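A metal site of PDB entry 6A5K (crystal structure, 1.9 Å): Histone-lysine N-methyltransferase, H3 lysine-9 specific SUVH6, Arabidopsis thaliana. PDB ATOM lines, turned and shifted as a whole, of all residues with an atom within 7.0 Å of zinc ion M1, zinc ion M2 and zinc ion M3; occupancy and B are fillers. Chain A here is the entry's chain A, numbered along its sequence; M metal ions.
SG of Cys 304 lies close to N of Cys 306 (3.4 Å).
N of Gly 333 lies close to SG of Cys 336, at 3.2 Å.
N of Lys 337 lies within hydrogen-bond range of O of Cys 290, at 3.2 Å.
N of Cys 332 sits at hydrogen-bond distance from O of Leu 344 (3.0 Å).
NH2 of Arg 345 sits close to O of Cys 336.
The side-chain sulfur (SG) of Cys 342 lies close to the backbone NH (N) of Leu 344 (3.2 Å).
O of Cys 338 lies within hydrogen-bond range of NH2 of Arg 345 (3.5 Å).
The side-chain sulfur (SG) of Cys 304 sits close to the backbone NH (N) of Val 307 (3.4 Å).
Within 4 Å of zinc ion M1: Cys 290, Cys 306, Cys 332 and Cys 336.
Along chain A the residues within 4 Å of zinc ion M1 span positions 290 to 336.
Four residues have an atom within 4 Å of zinc ion M2: Cys 296, Cys 332, Cys 338 and Cys 342.
The nearest printed residue that does not touch zinc ion M2 is Cys 290 (4.1 Å).
Four residues have an atom within 4 Å of zinc ion M3: Cys 290, Cys 292, Cys 296 and Cys 304.
The nearest printed residue that does not touch zinc ion M3 is Cys 332 (4.4 Å).
Zinc ion M1 is bound by the side-chain sulfur (SG) of Cys 306 (2.3 Å), the side-chain sulfur (SG) of Cys 336 (2.3 Å), the side-chain sulfur (SG) of Cys 290 (2.4 Å) and the side-chain sulfur (SG) of Cys 332 (2.4 Å).
Zinc ion M2 is bound by the side-chain sulfur (SG) of Cys 338 (2.3 Å), the side-chain sulfur (SG) of Cys 296 (2.4 Å), the side-chain sulfur (SG) of Cys 342 (2.4 Å) and the side-chain sulfur (SG) of Cys 332 (2.4 Å).
Zinc ion M2 has four donor atoms within binding distance.
SG of Cys 296 binds zinc ion M3, at 2.3 Å.
The side-chain sulfur (SG) of Cys 304 binds zinc ion M3.
Zinc ion M3 is bound by the side-chain sulfur (SG) of Cys 292 (2.5 Å).
SG of Cys 290 binds zinc ion M3, 2.5 Å away.
Zinc ion M3 has four donor atoms within binding distance.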
ATOM      1  N   LYS A 288     -34.651  20.549  11.000  1.00  0.00           N
ATOM      2  CA  LYS A 288     -33.521  21.047  10.231  1.00  0.00           C
ATOM      3  C   LYS A 288     -32.455  21.551  11.194  1.00  0.00           C
ATOM      4  O   LYS A 288     -32.756  22.248  12.161  1.00  0.00           O
ATOM      5  CB  LYS A 288     -33.947  22.154   9.271  1.00  0.00           C
ATOM      6  CG  LYS A 288     -32.879  22.540   8.256  1.00  0.00           C
ATOM      7  CD  LYS A 288     -33.018  23.983   7.808  1.00  0.00           C
ATOM      8  CE  LYS A 288     -32.072  24.300   6.657  1.00  0.00           C
ATOM      9  NZ  LYS A 288     -30.668  23.909   6.962  1.00  0.00           N
ATOM     10  N   SER A 289     -31.192  21.196  10.935  1.00  0.00           N
ATOM     11  CA  SER A 289     -30.111  21.618  11.818  1.00  0.00           C
ATOM     12  C   SER A 289     -29.142  22.560  11.108  1.00  0.00           C
ATOM     13  O   SER A 289     -29.175  22.688   9.882  1.00  0.00           O
ATOM     14  CB  SER A 289     -29.378  20.396  12.366  1.00  0.00           C
ATOM     15  OG  SER A 289     -28.897  19.582  11.299  1.00  0.00           O
ATOM     16  N   CYS A 290     -28.288  23.215  11.887  1.00  0.00           N
ATOM     17  CA  CYS A 290     -27.325  24.164  11.332  1.00  0.00           C
ATOM     18  C   CYS A 290     -25.938  23.535  11.232  1.00  0.00           C
ATOM     19  O   CYS A 290     -25.665  22.535  11.900  1.00  0.00           O
ATOM     20  CB  CYS A 290     -27.271  25.446  12.173  1.00  0.00           C
ATOM     21  SG  CYS A 290     -26.457  25.267  13.777  1.00  0.00           S
ATOM     22  N   CYS A 291     -25.071  24.113  10.409  1.00  0.00           N
ATOM     23  CA  CYS A 291     -23.757  23.539  10.174  1.00  0.00           C
ATOM     24  C   CYS A 291     -22.637  24.304  10.880  1.00  0.00           C
ATOM     25  O   CYS A 291     -21.456  24.093  10.606  1.00  0.00           O
ATOM     26  CB  CYS A 291     -23.472  23.480   8.671  1.00  0.00           C
ATOM     27  SG  CYS A 291     -23.635  25.038   7.782  1.00  0.00           S
ATOM     28  N   CYS A 292     -23.007  25.170  11.816  1.00  0.00           N
ATOM     29  CA  CYS A 292     -22.045  25.970  12.562  1.00  0.00           C
ATOM     30  C   CYS A 292     -21.212  25.100  13.488  1.00  0.00           C
ATOM     31  O   CYS A 292     -21.746  24.272  14.221  1.00  0.00           O
ATOM     32  CB  CYS A 292     -22.756  27.046  13.370  1.00  0.00           C
ATOM     33  SG  CYS A 292     -23.822  28.090  12.367  1.00  0.00           S
ATOM     34  N   THR A 293     -19.891  25.282  13.468  1.00  0.00           N
ATOM     35  CA  THR A 293     -19.021  24.505  14.339  1.00  0.00           C
ATOM     36  C   THR A 293     -18.708  25.275  15.616  1.00  0.00           C
ATOM     37  O   THR A 293     -18.350  24.683  16.634  1.00  0.00           O
ATOM     38  CB  THR A 293     -17.694  24.123  13.634  1.00  0.00           C
ATOM     39  OG1 THR A 293     -17.012  25.308  13.208  1.00  0.00           O
ATOM     40  CG2 THR A 293     -17.973  23.255  12.429  1.00  0.00           C
ATOM     41  N   THR A 294     -18.874  26.593  15.565  1.00  0.00           N
ATOM     42  CA  THR A 294     -18.704  27.426  16.750  1.00  0.00           C
ATOM     43  C   THR A 294     -20.074  27.878  17.255  1.00  0.00           C
ATOM     44  O   THR A 294     -21.109  27.521  16.669  1.00  0.00           O
ATOM     45  CB  THR A 294     -17.827  28.672  16.468  1.00  0.00           C
ATOM     46  OG1 THR A 294     -18.529  29.583  15.625  1.00  0.00           O
ATOM     47  CG2 THR A 294     -16.518  28.260  15.792  1.00  0.00           C
ATOM     48  N   ARG A 295     -20.099  28.674  18.300  1.00  0.00           N
ATOM     49  CA  ARG A 295     -21.354  29.185  18.838  1.00  0.00           C
ATOM     50  C   ARG A 295     -22.067  30.091  17.818  1.00  0.00           C
ATOM     51  O   ARG A 295     -21.464  30.948  17.239  1.00  0.00           O
ATOM     52  CB  ARG A 295     -21.069  29.863  20.191  1.00  0.00           C
ATOM     53  CG  ARG A 295     -20.687  28.918  21.321  1.00  0.00           C
ATOM     54  CD  ARG A 295     -20.340  29.643  22.613  1.00  0.00           C
ATOM     55  NE  ARG A 295     -19.481  30.783  22.370  1.00  0.00           N
ATOM     56  CZ  ARG A 295     -18.863  31.453  23.335  1.00  0.00           C
ATOM     57  NH1 ARG A 295     -18.053  32.446  23.046  1.00  0.00           N
ATOM     58  NH2 ARG A 295     -19.063  31.112  24.592  1.00  0.00           N
ATOM     59  N   CYS A 296     -23.379  29.925  17.647  1.00  0.00           N
ATOM     60  CA  CYS A 296     -24.149  30.753  16.707  1.00  0.00           C
ATOM     61  C   CYS A 296     -24.420  32.159  17.103  1.00  0.00           C
ATOM     62  O   CYS A 296     -24.801  32.401  18.171  1.00  0.00           O
ATOM     63  CB  CYS A 296     -25.406  29.900  16.307  1.00  0.00           C
ATOM     64  SG  CYS A 296     -25.167  28.107  16.018  1.00  0.00           S
ATOM     65  N   THR A 297     -24.207  33.044  16.162  1.00  0.00           N
ATOM     66  CA  THR A 297     -24.323  34.480  16.321  1.00  0.00           C
ATOM     67  C   THR A 297     -24.979  35.150  15.081  1.00  0.00           C
ATOM     68  O   THR A 297     -25.017  34.590  14.058  1.00  0.00           O
ATOM     69  CB  THR A 297     -22.911  35.131  16.635  1.00  0.00           C
ATOM     70  OG1 THR A 297     -22.103  35.127  15.481  1.00  0.00           O
ATOM     71  CG2 THR A 297     -22.092  34.487  17.818  1.00  0.00           C
ATOM     72  N   VAL A 303     -25.988  32.317   6.912  1.00  0.00           N
ATOM     73  CA  VAL A 303     -24.998  31.290   7.258  1.00  0.00           C
ATOM     74  C   VAL A 303     -25.594  30.238   8.195  1.00  0.00           C
ATOM     75  O   VAL A 303     -25.494  29.039   7.926  1.00  0.00           O
ATOM     76  CB  VAL A 303     -23.757  31.920   7.908  1.00  0.00           C
ATOM     77  CG1 VAL A 303     -22.772  30.838   8.342  1.00  0.00           C
ATOM     78  CG2 VAL A 303     -23.078  32.895   6.947  1.00  0.00           C
ATOM     79  N   CYS A 304     -26.212  30.689   9.280  1.00  0.00           N
ATOM     80  CA  CYS A 304     -26.803  29.780  10.260  1.00  0.00           C
ATOM     81  C   CYS A 304     -28.314  29.654  10.072  1.00  0.00           C
ATOM     82  O   CYS A 304     -29.041  30.651  10.172  1.00  0.00           O
ATOM     83  CB  CYS A 304     -26.502  30.234  11.688  1.00  0.00           C
ATOM     84  SG  CYS A 304     -27.351  29.251  12.950  1.00  0.00           S
ATOM     85  N   ALA A 305     -28.771  28.436   9.817  1.00  0.00           N
ATOM     86  CA  ALA A 305     -30.184  28.176   9.581  1.00  0.00           C
ATOM     87  C   ALA A 305     -31.035  28.518  10.803  1.00  0.00           C
ATOM     88  O   ALA A 305     -32.176  28.972  10.679  1.00  0.00           O
ATOM     89  CB  ALA A 305     -30.395  26.716   9.194  1.00  0.00           C
ATOM     90  N   CYS A 306     -30.477  28.295  11.993  1.00  0.00           N
ATOM     91  CA  CYS A 306     -31.234  28.462  13.220  1.00  0.00           C
ATOM     92  C   CYS A 306     -31.390  29.940  13.563  1.00  0.00           C
ATOM     93  O   CYS A 306     -32.413  30.348  14.107  1.00  0.00           O
ATOM     94  CB  CYS A 306     -30.554  27.684  14.337  1.00  0.00           C
ATOM     95  SG  CYS A 306     -30.449  25.913  13.937  1.00  0.00           S
ATOM     96  N   VAL A 307     -30.380  30.738  13.251  1.00  0.00           N
ATOM     97  CA  VAL A 307     -30.485  32.181  13.368  1.00  0.00           C
ATOM     98  C   VAL A 307     -31.586  32.675  12.433  1.00  0.00           C
ATOM     99  O   VAL A 307     -32.368  33.567  12.777  1.00  0.00           O
ATOM    100  CB  VAL A 307     -29.157  32.889  13.033  1.00  0.00           C
ATOM    101  CG1 VAL A 307     -29.343  34.401  12.916  1.00  0.00           C
ATOM    102  CG2 VAL A 307     -28.104  32.542  14.068  1.00  0.00           C
ATOM    103  N   LYS A 309     -34.203  30.940  11.371  1.00  0.00           N
ATOM    104  CA  LYS A 309     -35.495  30.580  11.954  1.00  0.00           C
ATOM    105  C   LYS A 309     -35.990  31.664  12.912  1.00  0.00           C
ATOM    106  O   LYS A 309     -37.184  31.963  12.974  1.00  0.00           O
ATOM    107  CB  LYS A 309     -35.395  29.243  12.714  1.00  0.00           C
ATOM    108  CG  LYS A 309     -35.169  28.020  11.847  1.00  0.00           C
ATOM    109  CD  LYS A 309     -35.268  26.748  12.697  1.00  0.00           C
ATOM    110  CE  LYS A 309     -34.554  25.566  12.054  1.00  0.00           C
ATOM    111  NZ  LYS A 309     -34.566  24.367  12.943  1.00  0.00           N
ATOM    112  N   GLU A 331     -34.335  27.048  19.323  1.00  0.00           N
ATOM    113  CA  GLU A 331     -33.009  26.715  19.813  1.00  0.00           C
ATOM    114  C   GLU A 331     -32.355  25.711  18.876  1.00  0.00           C
ATOM    115  O   GLU A 331     -33.042  25.041  18.104  1.00  0.00           O
ATOM    116  CB  GLU A 331     -33.073  26.163  21.234  1.00  0.00           C
ATOM    117  CG  GLU A 331     -33.554  27.180  22.264  1.00  0.00           C
ATOM    118  CD  GLU A 331     -33.329  26.725  23.692  1.00  0.00           C
ATOM    119  OE1 GLU A 331     -32.641  25.697  23.900  1.00  0.00           O
ATOM    120  OE2 GLU A 331     -33.824  27.406  24.607  1.00  0.00           O
ATOM    121  N   CYS A 332     -31.036  25.622  18.932  1.00  0.00           N
ATOM    122  CA  CYS A 332     -30.332  24.605  18.169  1.00  0.00           C
ATOM    123  C   CYS A 332     -30.687  23.222  18.698  1.00  0.00           C
ATOM    124  O   CYS A 332     -30.978  23.061  19.887  1.00  0.00           O
ATOM    125  CB  CYS A 332     -28.829  24.853  18.197  1.00  0.00           C
ATOM    126  SG  CYS A 332     -28.369  26.234  17.167  1.00  0.00           S
ATOM    127  N   GLY A 333     -30.688  22.240  17.807  1.00  0.00           N
ATOM    128  CA  GLY A 333     -31.148  20.910  18.135  1.00  0.00           C
ATOM    129  C   GLY A 333     -30.048  19.874  18.232  1.00  0.00           C
ATOM    130  O   GLY A 333     -28.858  20.212  18.199  1.00  0.00           O
ATOM    131  N   LEU A 335     -28.867  17.657  16.188  1.00  0.00           N
ATOM    132  CA  LEU A 335     -27.963  17.437  15.061  1.00  0.00           C
ATOM    133  C   LEU A 335     -27.223  18.704  14.617  1.00  0.00           C
ATOM    134  O   LEU A 335     -26.480  18.670  13.633  1.00  0.00           O
ATOM    135  CB  LEU A 335     -28.741  16.861  13.870  1.00  0.00           C
ATOM    136  CG  LEU A 335     -29.376  15.480  14.042  1.00  0.00           C
ATOM    137  CD1 LEU A 335     -29.660  14.857  12.684  1.00  0.00           C
ATOM    138  CD2 LEU A 335     -28.487  14.576  14.887  1.00  0.00           C
ATOM    139  N   CYS A 336     -27.432  19.814  15.330  1.00  0.00           N
ATOM    140  CA  CYS A 336     -26.685  21.040  15.054  1.00  0.00           C
ATOM    141  C   CYS A 336     -25.207  20.830  15.406  1.00  0.00           C
ATOM    142  O   CYS A 336     -24.894  20.276  16.452  1.00  0.00           O
ATOM    143  CB  CYS A 336     -27.249  22.223  15.833  1.00  0.00           C
ATOM    144  SG  CYS A 336     -28.830  22.878  15.232  1.00  0.00           S
ATOM    145  N   LYS A 337     -24.304  21.278  14.528  1.00  0.00           N
ATOM    146  CA  LYS A 337     -22.880  21.015  14.704  1.00  0.00           C
ATOM    147  C   LYS A 337     -22.272  21.873  15.824  1.00  0.00           C
ATOM    148  O   LYS A 337     -21.133  21.654  16.215  1.00  0.00           O
ATOM    149  CB  LYS A 337     -22.105  21.269  13.402  1.00  0.00           C
ATOM    150  CG  LYS A 337     -22.621  20.533  12.172  1.00  0.00           C
ATOM    151  CD  LYS A 337     -21.697  20.808  10.991  1.00  0.00           C
ATOM    152  CE  LYS A 337     -21.956  19.892   9.811  1.00  0.00           C
ATOM    153  NZ  LYS A 337     -21.062  20.242   8.658  1.00  0.00           N
ATOM    154  N   CYS A 338     -23.033  22.855  16.300  1.00  0.00           N
ATOM    155  CA  CYS A 338     -22.531  23.797  17.293  1.00  0.00           C
ATOM    156  C   CYS A 338     -22.320  23.143  18.661  1.00  0.00           C
ATOM    157  O   CYS A 338     -22.955  22.135  18.978  1.00  0.00           O
ATOM    158  CB  CYS A 338     -23.510  24.969  17.417  1.00  0.00           C
ATOM    159  SG  CYS A 338     -25.160  24.445  17.872  1.00  0.00           S
ATOM    160  N   PRO A 339     -21.421  23.708  19.479  1.00  0.00           N
ATOM    161  CA  PRO A 339     -21.184  23.121  20.798  1.00  0.00           C
ATOM    162  C   PRO A 339     -22.360  23.321  21.764  1.00  0.00           C
ATOM    163  O   PRO A 339     -23.279  24.101  21.503  1.00  0.00           O
ATOM    164  CB  PRO A 339     -19.944  23.872  21.300  1.00  0.00           C
ATOM    165  CG  PRO A 339     -19.975  25.171  20.556  1.00  0.00           C
ATOM    166  CD  PRO A 339     -20.524  24.847  19.208  1.00  0.00           C
ATOM    167  N   CYS A 342     -23.487  26.743  22.879  1.00  0.00           N
ATOM    168  CA  CYS A 342     -24.096  27.621  21.886  1.00  0.00           C
ATOM    169  C   CYS A 342     -25.098  28.571  22.529  1.00  0.00           C
ATOM    170  O   CYS A 342     -25.889  28.166  23.372  1.00  0.00           O
ATOM    171  CB  CYS A 342     -24.809  26.816  20.796  1.00  0.00           C
ATOM    172  SG  CYS A 342     -25.691  27.883  19.623  1.00  0.00           S
ATOM    173  N   TYR A 343     -25.040  29.830  22.096  1.00  0.00           N
ATOM    174  CA  TYR A 343     -25.930  30.853  22.644  1.00  0.00           C
ATOM    175  C   TYR A 343     -27.404  30.518  22.403  1.00  0.00           C
ATOM    176  O   TYR A 343     -28.290  30.997  23.116  1.00  0.00           O
ATOM    177  CB  TYR A 343     -25.576  32.213  22.018  1.00  0.00           C
ATOM    178  CG  TYR A 343     -24.163  32.652  22.339  1.00  0.00           C
ATOM    179  CD1 TYR A 343     -23.702  32.681  23.649  1.00  0.00           C
ATOM    180  CD2 TYR A 343     -23.278  33.019  21.327  1.00  0.00           C
ATOM    181  CE1 TYR A 343     -22.411  33.082  23.961  1.00  0.00           C
ATOM    182  CE2 TYR A 343     -21.983  33.426  21.627  1.00  0.00           C
ATOM    183  CZ  TYR A 343     -21.558  33.450  22.945  1.00  0.00           C
ATOM    184  OH  TYR A 343     -20.285  33.856  23.244  1.00  0.00           O
ATOM    185  N   LEU A 344     -27.648  29.673  21.403  1.00  0.00           N
ATOM    186  CA  LEU A 344     -28.992  29.199  21.108  1.00  0.00           C
ATOM    187  C   LEU A 344     -29.313  27.856  21.773  1.00  0.00           C
ATOM    188  O   LEU A 344     -30.201  27.143  21.331  1.00  0.00           O
ATOM    189  CB  LEU A 344     -29.183  29.068  19.598  1.00  0.00           C
ATOM    190  CG  LEU A 344     -29.193  30.368  18.804  1.00  0.00           C
ATOM    191  CD1 LEU A 344     -29.412  30.066  17.319  1.00  0.00           C
ATOM    192  CD2 LEU A 344     -30.272  31.294  19.344  1.00  0.00           C
ATOM    193  N   ARG A 345     -28.580  27.510  22.824  1.00  0.00           N
ATOM    194  CA  ARG A 345     -28.945  26.346  23.634  1.00  0.00           C
ATOM    195  C   ARG A 345     -29.102  26.784  25.082  1.00  0.00           C
ATOM    196  O   ARG A 345     -28.124  26.974  25.793  1.00  0.00           O
ATOM    197  CB  ARG A 345     -27.887  25.242  23.517  1.00  0.00           C
ATOM    198  CG  ARG A 345     -27.709  24.664  22.131  1.00  0.00           C
ATOM    199  CD  ARG A 345     -26.693  23.526  22.167  1.00  0.00           C
ATOM    200  NE  ARG A 345     -26.269  23.080  20.847  1.00  0.00           N
ATOM    201  CZ  ARG A 345     -26.867  22.102  20.169  1.00  0.00           C
ATOM    202  NH1 ARG A 345     -27.939  21.496  20.692  1.00  0.00           N
ATOM    203  NH2 ARG A 345     -26.412  21.742  18.983  1.00  0.00           N
HETATM  204 ZN    ZN M   1     -28.521  25.196  15.000  1.00  0.00          ZN
HETATM  205 ZN    ZN M   2     -26.032  26.589  17.627  1.00  0.00          ZN
HETATM  206 ZN    ZN M   3     -25.852  27.729  13.840  1.00  0.00          ZN
